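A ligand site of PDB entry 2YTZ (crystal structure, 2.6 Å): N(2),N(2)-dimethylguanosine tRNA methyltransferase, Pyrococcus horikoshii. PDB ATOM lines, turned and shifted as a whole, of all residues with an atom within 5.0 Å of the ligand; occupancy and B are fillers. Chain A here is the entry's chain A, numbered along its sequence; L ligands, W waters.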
ATOM      1  N   PHE A  27       2.812 -15.314   6.268  1.00  0.00           N
ATOM      2  CA  PHE A  27       3.801 -16.326   5.937  1.00  0.00           C
ATOM      3  C   PHE A  27       4.491 -16.142   4.591  1.00  0.00           C
ATOM      4  O   PHE A  27       3.890 -15.719   3.610  1.00  0.00           O
ATOM      5  CB  PHE A  27       3.184 -17.719   5.970  1.00  0.00           C
ATOM      6  CG  PHE A  27       4.195 -18.822   5.891  1.00  0.00           C
ATOM      7  CD1 PHE A  27       4.841 -19.287   7.039  1.00  0.00           C
ATOM      8  CD2 PHE A  27       4.523 -19.389   4.662  1.00  0.00           C
ATOM      9  CE1 PHE A  27       5.806 -20.294   6.967  1.00  0.00           C
ATOM     10  CE2 PHE A  27       5.499 -20.400   4.582  1.00  0.00           C
ATOM     11  CZ  PHE A  27       6.134 -20.848   5.743  1.00  0.00           C
ATOM     12  N   TYR A  28       5.777 -16.468   4.583  1.00  0.00           N
ATOM     13  CA  TYR A  28       6.601 -16.411   3.384  1.00  0.00           C
ATOM     14  C   TYR A  28       7.873 -17.214   3.586  1.00  0.00           C
ATOM     15  O   TYR A  28       8.743 -16.800   4.346  1.00  0.00           O
ATOM     16  CB  TYR A  28       7.002 -14.981   3.025  1.00  0.00           C
ATOM     17  CG  TYR A  28       7.970 -14.968   1.863  1.00  0.00           C
ATOM     18  CD1 TYR A  28       7.545 -15.250   0.565  1.00  0.00           C
ATOM     19  CD2 TYR A  28       9.330 -14.727   2.072  1.00  0.00           C
ATOM     20  CE1 TYR A  28       8.445 -15.294  -0.492  1.00  0.00           C
ATOM     21  CE2 TYR A  28      10.238 -14.781   1.021  1.00  0.00           C
ATOM     22  CZ  TYR A  28       9.792 -15.066  -0.267  1.00  0.00           C
ATOM     23  OH  TYR A  28      10.697 -15.134  -1.301  1.00  0.00           O
ATOM     24  N   ARG A  36       8.151 -22.577  -6.562  1.00  0.00           N
ATOM     25  CA  ARG A  36       7.421 -21.639  -7.423  1.00  0.00           C
ATOM     26  C   ARG A  36       8.071 -21.492  -8.790  1.00  0.00           C
ATOM     27  O   ARG A  36       7.394 -21.173  -9.778  1.00  0.00           O
ATOM     28  CB  ARG A  36       7.281 -20.284  -6.731  1.00  0.00           C
ATOM     29  CG  ARG A  36       6.362 -20.325  -5.496  1.00  0.00           C
ATOM     30  CD  ARG A  36       6.167 -18.961  -4.848  1.00  0.00           C
ATOM     31  NE  ARG A  36       7.347 -18.496  -4.119  1.00  0.00           N
ATOM     32  CZ  ARG A  36       7.611 -18.798  -2.845  1.00  0.00           C
ATOM     33  NH1 ARG A  36       6.787 -19.567  -2.155  1.00  0.00           N
ATOM     34  NH2 ARG A  36       8.711 -18.322  -2.263  1.00  0.00           N
ATOM     35  N   ASP A  53      -4.369 -19.204  -7.138  1.00  0.00           N
ATOM     36  CA  ASP A  53      -3.396 -19.421  -6.064  1.00  0.00           C
ATOM     37  C   ASP A  53      -4.297 -19.521  -4.833  1.00  0.00           C
ATOM     38  O   ASP A  53      -4.520 -18.535  -4.130  1.00  0.00           O
ATOM     39  CB  ASP A  53      -2.452 -18.207  -5.970  1.00  0.00           C
ATOM     40  CG  ASP A  53      -1.396 -18.349  -4.876  1.00  0.00           C
ATOM     41  OD1 ASP A  53      -1.322 -19.424  -4.225  1.00  0.00           O
ATOM     42  OD2 ASP A  53      -0.635 -17.388  -4.656  1.00  0.00           O
ATOM     43  N   ALA A  54      -4.823 -20.720  -4.579  1.00  0.00           N
ATOM     44  CA  ALA A  54      -5.748 -20.987  -3.464  1.00  0.00           C
ATOM     45  C   ALA A  54      -5.411 -20.359  -2.122  1.00  0.00           C
ATOM     46  O   ALA A  54      -6.244 -19.688  -1.523  1.00  0.00           O
ATOM     47  CB  ALA A  54      -5.945 -22.493  -3.301  1.00  0.00           C
ATOM     48  N   LEU A  55      -4.197 -20.592  -1.629  1.00  0.00           N
ATOM     49  CA  LEU A  55      -3.765 -20.033  -0.345  1.00  0.00           C
ATOM     50  C   LEU A  55      -2.544 -19.160  -0.640  1.00  0.00           C
ATOM     51  O   LEU A  55      -1.395 -19.591  -0.496  1.00  0.00           O
ATOM     52  CB  LEU A  55      -3.444 -21.176   0.617  1.00  0.00           C
ATOM     53  CG  LEU A  55      -4.595 -22.188   0.784  1.00  0.00           C
ATOM     54  CD1 LEU A  55      -4.518 -23.207  -0.339  1.00  0.00           C
ATOM     55  CD2 LEU A  55      -4.504 -22.902   2.123  1.00  0.00           C
ATOM     56  N   SER A  56      -2.826 -17.919  -1.036  1.00  0.00           N
ATOM     57  CA  SER A  56      -1.816 -16.954  -1.451  1.00  0.00           C
ATOM     58  C   SER A  56      -0.826 -16.317  -0.446  1.00  0.00           C
ATOM     59  O   SER A  56       0.294 -16.005  -0.823  1.00  0.00           O
ATOM     60  CB  SER A  56      -2.538 -15.850  -2.231  1.00  0.00           C
ATOM     61  OG  SER A  56      -1.703 -15.337  -3.256  1.00  0.00           O
ATOM     62  N   ALA A  57      -1.219 -16.137   0.805  1.00  0.00           N
ATOM     63  CA  ALA A  57      -0.328 -15.507   1.791  1.00  0.00           C
ATOM     64  C   ALA A  57       0.121 -14.111   1.287  1.00  0.00           C
ATOM     65  O   ALA A  57      -0.704 -13.205   1.188  1.00  0.00           O
ATOM     66  CB  ALA A  57       0.879 -16.392   2.065  1.00  0.00           C
ATOM     67  N   THR A  58       1.408 -13.936   0.968  1.00  0.00           N
ATOM     68  CA  THR A  58       1.889 -12.633   0.486  1.00  0.00           C
ATOM     69  C   THR A  58       1.412 -12.322  -0.926  1.00  0.00           C
ATOM     70  O   THR A  58       1.454 -11.180  -1.363  1.00  0.00           O
ATOM     71  CB  THR A  58       3.435 -12.553   0.448  1.00  0.00           C
ATOM     72  OG1 THR A  58       3.938 -13.493  -0.508  1.00  0.00           O
ATOM     73  CG2 THR A  58       4.031 -12.840   1.819  1.00  0.00           C
ATOM     74  N   ILE A  60       2.772 -13.782  -3.491  1.00  0.00           N
ATOM     75  CA  ILE A  60       3.934 -14.021  -4.322  1.00  0.00           C
ATOM     76  C   ILE A  60       3.723 -15.011  -5.479  1.00  0.00           C
ATOM     77  O   ILE A  60       4.076 -14.733  -6.619  1.00  0.00           O
ATOM     78  CB  ILE A  60       5.134 -14.472  -3.449  1.00  0.00           C
ATOM     79  CG1 ILE A  60       6.337 -14.813  -4.328  1.00  0.00           C
ATOM     80  CG2 ILE A  60       4.740 -15.660  -2.602  1.00  0.00           C
ATOM     81  CD1 ILE A  60       6.772 -13.688  -5.209  1.00  0.00           C
ATOM     82  N   ARG A  61       3.132 -16.169  -5.173  1.00  0.00           N
ATOM     83  CA  ARG A  61       2.880 -17.192  -6.188  1.00  0.00           C
ATOM     84  C   ARG A  61       2.015 -16.644  -7.331  1.00  0.00           C
ATOM     85  O   ARG A  61       2.437 -16.624  -8.492  1.00  0.00           O
ATOM     86  CB  ARG A  61       2.178 -18.395  -5.534  1.00  0.00           C
ATOM     87  CG  ARG A  61       2.137 -19.672  -6.346  1.00  0.00           C
ATOM     88  CD  ARG A  61       1.631 -20.812  -5.467  1.00  0.00           C
ATOM     89  NE  ARG A  61       2.544 -21.144  -4.371  1.00  0.00           N
ATOM     90  CZ  ARG A  61       3.460 -22.108  -4.434  1.00  0.00           C
ATOM     91  NH1 ARG A  61       4.254 -22.351  -3.391  1.00  0.00           N
ATOM     92  NH2 ARG A  61       3.579 -22.848  -5.533  1.00  0.00           N
ATOM     93  N   ASN A  77      -6.003 -15.667  -3.282  1.00  0.00           N
ATOM     94  CA  ASN A  77      -6.929 -15.808  -2.179  1.00  0.00           C
ATOM     95  C   ASN A  77      -6.229 -16.217  -0.885  1.00  0.00           C
ATOM     96  O   ASN A  77      -5.236 -16.941  -0.904  1.00  0.00           O
ATOM     97  CB  ASN A  77      -7.994 -16.860  -2.513  1.00  0.00           C
ATOM     98  CG  ASN A  77      -8.952 -17.109  -1.365  1.00  0.00           C
ATOM     99  OD1 ASN A  77      -9.898 -16.344  -1.162  1.00  0.00           O
ATOM    100  ND2 ASN A  77      -8.692 -18.164  -0.593  1.00  0.00           N
ATOM    101  N   ASP A  78      -6.748 -15.719   0.232  1.00  0.00           N
ATOM    102  CA  ASP A  78      -6.248 -16.065   1.542  1.00  0.00           C
ATOM    103  C   ASP A  78      -7.320 -15.729   2.571  1.00  0.00           C
ATOM    104  O   ASP A  78      -8.026 -14.729   2.443  1.00  0.00           O
ATOM    105  CB  ASP A  78      -4.948 -15.329   1.866  1.00  0.00           C
ATOM    106  CG  ASP A  78      -4.097 -16.098   2.875  1.00  0.00           C
ATOM    107  OD1 ASP A  78      -3.085 -16.707   2.467  1.00  0.00           O
ATOM    108  OD2 ASP A  78      -4.454 -16.106   4.081  1.00  0.00           O
ATOM    109  N   ILE A  79      -7.435 -16.568   3.591  1.00  0.00           N
ATOM    110  CA  ILE A  79      -8.425 -16.393   4.623  1.00  0.00           C
ATOM    111  C   ILE A  79      -8.032 -15.337   5.650  1.00  0.00           C
ATOM    112  O   ILE A  79      -8.883 -14.834   6.387  1.00  0.00           O
ATOM    113  CB  ILE A  79      -8.672 -17.717   5.371  1.00  0.00           C
ATOM    114  CG1 ILE A  79     -10.003 -17.636   6.121  1.00  0.00           C
ATOM    115  CG2 ILE A  79      -7.527 -18.009   6.343  1.00  0.00           C
ATOM    116  CD1 ILE A  79     -10.398 -18.935   6.786  1.00  0.00           C
ATOM    117  N   SER A  80      -6.743 -14.989   5.683  1.00  0.00           N
ATOM    118  CA  SER A  80      -6.252 -14.001   6.630  1.00  0.00           C
ATOM    119  C   SER A  80      -6.370 -12.548   6.159  1.00  0.00           C
ATOM    120  O   SER A  80      -5.996 -12.210   5.038  1.00  0.00           O
ATOM    121  CB  SER A  80      -4.787 -14.274   6.970  1.00  0.00           C
ATOM    122  OG  SER A  80      -4.267 -13.211   7.744  1.00  0.00           O
ATOM    123  N   ALA A  83      -3.054 -10.971   5.389  1.00  0.00           N
ATOM    124  CA  ALA A  83      -2.509 -11.504   4.146  1.00  0.00           C
ATOM    125  C   ALA A  83      -3.193 -10.794   2.996  1.00  0.00           C
ATOM    126  O   ALA A  83      -2.543 -10.334   2.050  1.00  0.00           O
ATOM    127  CB  ALA A  83      -2.764 -13.011   4.061  1.00  0.00           C
ATOM    128  N   ASP A 119     -11.026 -14.610   1.440  1.00  0.00           N
ATOM    129  CA  ASP A 119     -12.016 -15.626   1.692  1.00  0.00           C
ATOM    130  C   ASP A 119     -11.405 -16.977   1.998  1.00  0.00           C
ATOM    131  O   ASP A 119     -10.202 -17.183   1.839  1.00  0.00           O
ATOM    132  CB  ASP A 119     -12.924 -15.730   0.449  1.00  0.00           C
ATOM    133  CG  ASP A 119     -14.204 -16.490   0.710  1.00  0.00           C
ATOM    134  OD1 ASP A 119     -14.561 -16.712   1.901  1.00  0.00           O
ATOM    135  OD2 ASP A 119     -14.886 -16.842  -0.288  1.00  0.00           O
ATOM    136  N   ASP A 120     -12.257 -17.894   2.464  1.00  0.00           N
ATOM    137  CA  ASP A 120     -11.860 -19.261   2.775  1.00  0.00           C
ATOM    138  C   ASP A 120     -11.789 -20.003   1.429  1.00  0.00           C
ATOM    139  O   ASP A 120     -12.715 -19.928   0.622  1.00  0.00           O
ATOM    140  CB  ASP A 120     -12.920 -19.879   3.701  1.00  0.00           C
ATOM    141  CG  ASP A 120     -12.857 -21.395   3.732  1.00  0.00           C
ATOM    142  OD1 ASP A 120     -11.780 -21.966   3.457  1.00  0.00           O
ATOM    143  OD2 ASP A 120     -13.887 -22.010   4.066  1.00  0.00           O
ATOM    144  N   ALA A 121     -10.672 -20.694   1.190  1.00  0.00           N
ATOM    145  CA  ALA A 121     -10.452 -21.422  -0.057  1.00  0.00           C
ATOM    146  C   ALA A 121     -11.595 -22.360  -0.428  1.00  0.00           C
ATOM    147  O   ALA A 121     -11.988 -22.440  -1.580  1.00  0.00           O
ATOM    148  CB  ALA A 121      -9.139 -22.201   0.007  1.00  0.00           C
ATOM    149  N   ASP A 138      -1.158 -24.952  -1.971  1.00  0.00           N
ATOM    150  CA  ASP A 138       0.089 -24.887  -1.234  1.00  0.00           C
ATOM    151  C   ASP A 138      -0.235 -24.579   0.232  1.00  0.00           C
ATOM    152  O   ASP A 138       0.004 -23.468   0.712  1.00  0.00           O
ATOM    153  CB  ASP A 138       0.952 -23.783  -1.848  1.00  0.00           C
ATOM    154  CG  ASP A 138       2.327 -23.703  -1.223  1.00  0.00           C
ATOM    155  OD1 ASP A 138       3.020 -24.744  -1.167  1.00  0.00           O
ATOM    156  OD2 ASP A 138       2.702 -22.593  -0.784  1.00  0.00           O
ATOM    157  N   PRO A 139      -0.792 -25.564   0.949  1.00  0.00           N
ATOM    158  CA  PRO A 139      -1.167 -25.394   2.360  1.00  0.00           C
ATOM    159  C   PRO A 139      -0.046 -25.721   3.346  1.00  0.00           C
ATOM    160  O   PRO A 139       1.034 -26.164   2.959  1.00  0.00           O
ATOM    161  CB  PRO A 139      -2.323 -26.369   2.510  1.00  0.00           C
ATOM    162  CG  PRO A 139      -1.804 -27.538   1.713  1.00  0.00           C
ATOM    163  CD  PRO A 139      -1.231 -26.879   0.450  1.00  0.00           C
ATOM    164  N   PHE A 140      -0.329 -25.499   4.623  1.00  0.00           N
ATOM    165  CA  PHE A 140       0.635 -25.808   5.660  1.00  0.00           C
ATOM    166  C   PHE A 140       0.535 -27.301   5.928  1.00  0.00           C
ATOM    167  O   PHE A 140      -0.278 -27.729   6.752  1.00  0.00           O
ATOM    168  CB  PHE A 140       0.320 -25.042   6.945  1.00  0.00           C
ATOM    169  CG  PHE A 140       0.671 -23.585   6.887  1.00  0.00           C
ATOM    170  CD1 PHE A 140       1.904 -23.186   6.386  1.00  0.00           C
ATOM    171  CD2 PHE A 140      -0.212 -22.636   7.379  1.00  0.00           C
ATOM    172  CE1 PHE A 140       2.252 -21.835   6.386  1.00  0.00           C
ATOM    173  CE2 PHE A 140       0.135 -21.285   7.379  1.00  0.00           C
ATOM    174  CZ  PHE A 140       1.368 -20.887   6.878  1.00  0.00           C
ATOM    175  N   PHE A 146      -8.790 -29.331   1.366  1.00  0.00           N
ATOM    176  CA  PHE A 146      -9.211 -28.600   0.158  1.00  0.00           C
ATOM    177  C   PHE A 146      -9.306 -29.436  -1.120  1.00  0.00           C
ATOM    178  O   PHE A 146      -9.984 -29.056  -2.069  1.00  0.00           O
ATOM    179  CB  PHE A 146      -8.220 -27.453  -0.120  1.00  0.00           C
ATOM    180  CG  PHE A 146      -7.959 -26.579   1.061  1.00  0.00           C
ATOM    181  CD1 PHE A 146      -8.889 -25.614   1.452  1.00  0.00           C
ATOM    182  CD2 PHE A 146      -6.784 -26.725   1.796  1.00  0.00           C
ATOM    183  CE1 PHE A 146      -8.631 -24.804   2.562  1.00  0.00           C
ATOM    184  CE2 PHE A 146      -6.516 -25.915   2.907  1.00  0.00           C
ATOM    185  CZ  PHE A 146      -7.445 -24.954   3.289  1.00  0.00           C
HETATM  186  N1  LIG L   1       1.231 -19.870  -1.487  1.00  0.00           N
HETATM  187  C1  LIG L   1       2.412 -19.529  -0.890  1.00  0.00           C
HETATM  188  C2  LIG L   1       2.022 -19.780   0.607  1.00  0.00           C
HETATM  189  C3  LIG L   1       1.117 -20.170   1.747  1.00  0.00           C
HETATM  190  S1  LIG L   1       1.120 -20.299   3.454  1.00  0.00           S
HETATM  191  C4  LIG L   1       3.688 -19.096  -1.325  1.00  0.00           C
HETATM  192  O1  LIG L   1       4.184 -18.243  -0.461  1.00  0.00           O
HETATM  193  O2  LIG L   1       4.173 -19.549  -2.400  1.00  0.00           O
HETATM  194  C5  LIG L   1      -0.448 -20.894   3.664  1.00  0.00           C
HETATM  195  C6  LIG L   1      -1.335 -19.854   4.368  1.00  0.00           C
HETATM  196  O3  LIG L   1      -2.607 -20.443   4.113  1.00  0.00           O
HETATM  197  C7  LIG L   1      -1.558 -18.496   4.994  1.00  0.00           C
HETATM  198  O4  LIG L   1      -1.301 -17.202   4.382  1.00  0.00           O
HETATM  199  C8  LIG L   1      -2.993 -18.557   5.488  1.00  0.00           C
HETATM  200  O5  LIG L   1      -3.641 -17.726   6.278  1.00  0.00           O
HETATM  201  C9  LIG L   1      -3.589 -19.815   4.902  1.00  0.00           C
HETATM  202  N2  LIG L   1      -4.993 -20.532   4.975  1.00  0.00           N
HETATM  203  C10 LIG L   1      -5.260 -21.443   5.889  1.00  0.00           C
HETATM  204  N3  LIG L   1      -6.469 -21.875   5.759  1.00  0.00           N
HETATM  205  C11 LIG L   1      -7.025 -21.247   4.758  1.00  0.00           C
HETATM  206  C12 LIG L   1      -8.289 -21.301   4.146  1.00  0.00           C
HETATM  207  N4  LIG L   1      -9.210 -22.135   4.633  1.00  0.00           N
HETATM  208  N5  LIG L   1      -8.580 -20.479   3.055  1.00  0.00           N
HETATM  209  C13 LIG L   1      -7.653 -19.612   2.543  1.00  0.00           C
HETATM  210  N6  LIG L   1      -6.414 -19.551   3.116  1.00  0.00           N
HETATM  211  C14 LIG L   1      -6.063 -20.354   4.216  1.00  0.00           C
HETATM  212  O   HOH W   1       6.379 -19.527   0.927  1.00  0.00           O
HETATM  213  O   HOH W   2       3.962 -15.869   0.946  1.00  0.00           O
HETATM  214  O   HOH W   3       1.392 -17.199  -2.842  1.00  0.00           O
HETATM  215  O   HOH W   4      -9.659 -24.209   6.637  1.00  0.00           O
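O of Leu 55 is in hydrogen-bond range of N1 of the ligand (2.8 Å).
An oxygen (O2) of the ligand is in salt-bridge range of the guanidinium group of Arg 36.
N1 of the ligand lies within salt-bridge range of OD2 of Asp 138 (3.2 Å).
The side-chain carboxylate (OD1) of Asp 78 sits at hydrogen-bond distance from an oxygen (O4) of the ligand (2.7 Å).
A nitrogen (N6) of the ligand is in hydrogen-bond range of the backbone NH (N) of Ile 79 (3.2 Å).
OD1 of Asp 53 is in salt-bridge range of N1 of the ligand, at 3.8 Å.
The guanidinium group (NH1) of Arg 61 is in salt-bridge range of an oxygen (O2) of the ligand.
OD1 of Asp 120 lies within hydrogen-bond range of N4 of the ligand, 2.8 Å away.
N of Ala 121 lies within hydrogen-bond range of N5 of the ligand (2.8 Å).
OD2 of Asp 138 lies within salt-bridge range of NH1 of Arg 61, 3.0 Å away.
N of Asp 119 lies within hydrogen-bond range of O of Asp 78.
The side-chain hydroxyl of Ser 56 sits at hydrogen-bond distance from the side-chain carboxylate of Asp 53, at 2.7 Å.
O of Asn 77 sits at hydrogen-bond distance from N of Ser 56, at 2.6 Å.
The backbone NH of Asn 77 sits at hydrogen-bond distance from the backbone carbonyl oxygen of Asp 53 (3.3 Å).
The side-chain hydroxyl (OG1) of Thr 58 sits close to the backbone NH (N) of Ile 60 (3.2 Å).
The side-chain hydroxyl of Ser 80 sits at hydrogen-bond distance from the backbone NH of Ala 83.
The backbone NH (N) of Ile 79 sits at hydrogen-bond distance from the backbone carbonyl oxygen (O) of Asp 119, 3.3 Å away.
Residues that only touch the ligand: Ala 57 (3.2 Å), Ile 60 (3.4 Å), Phe 146 (3.4 Å), Phe 140 (3.5 Å), Asp 119 (3.6 Å), Asn 77 (3.6 Å), Ser 80 (3.7 Å) and Phe 27 (3.7 Å).
17 residues have an atom within 4 Å of the ligand: Phe 27, Arg 36, Asp 53, Leu 55, Ala 57, Ile 60, Arg 61, Asn 77, Asp 78, Ile 79, Ser 80, Asp 119, Asp 120, Ala 121, Asp 138, Phe 140 and Phe 146.
Along chain A the residues within 4 Å of the ligand span positions 27 to 146.
The nearest printed residue that does not touch the ligand is Ser 56 (4.03 Å).
Water W2 lies within hydrogen-bond range of the backbone carbonyl oxygen of Phe 27 (2.7 Å), an oxygen (O1) of the ligand (2.8 Å) and the side-chain hydroxyl of Thr 58 (2.8 Å).
Water W1 bridges an oxygen (O1) of the ligand and the guanidinium group (NH1) of Arg 36.
Water W3 lies within hydrogen-bond range of O of Ser 56 (2.6 Å), OD2 of Asp 53 (2.7 Å), N1 of the ligand (3.0 Å) and N of Arg 61 (3.1 Å).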
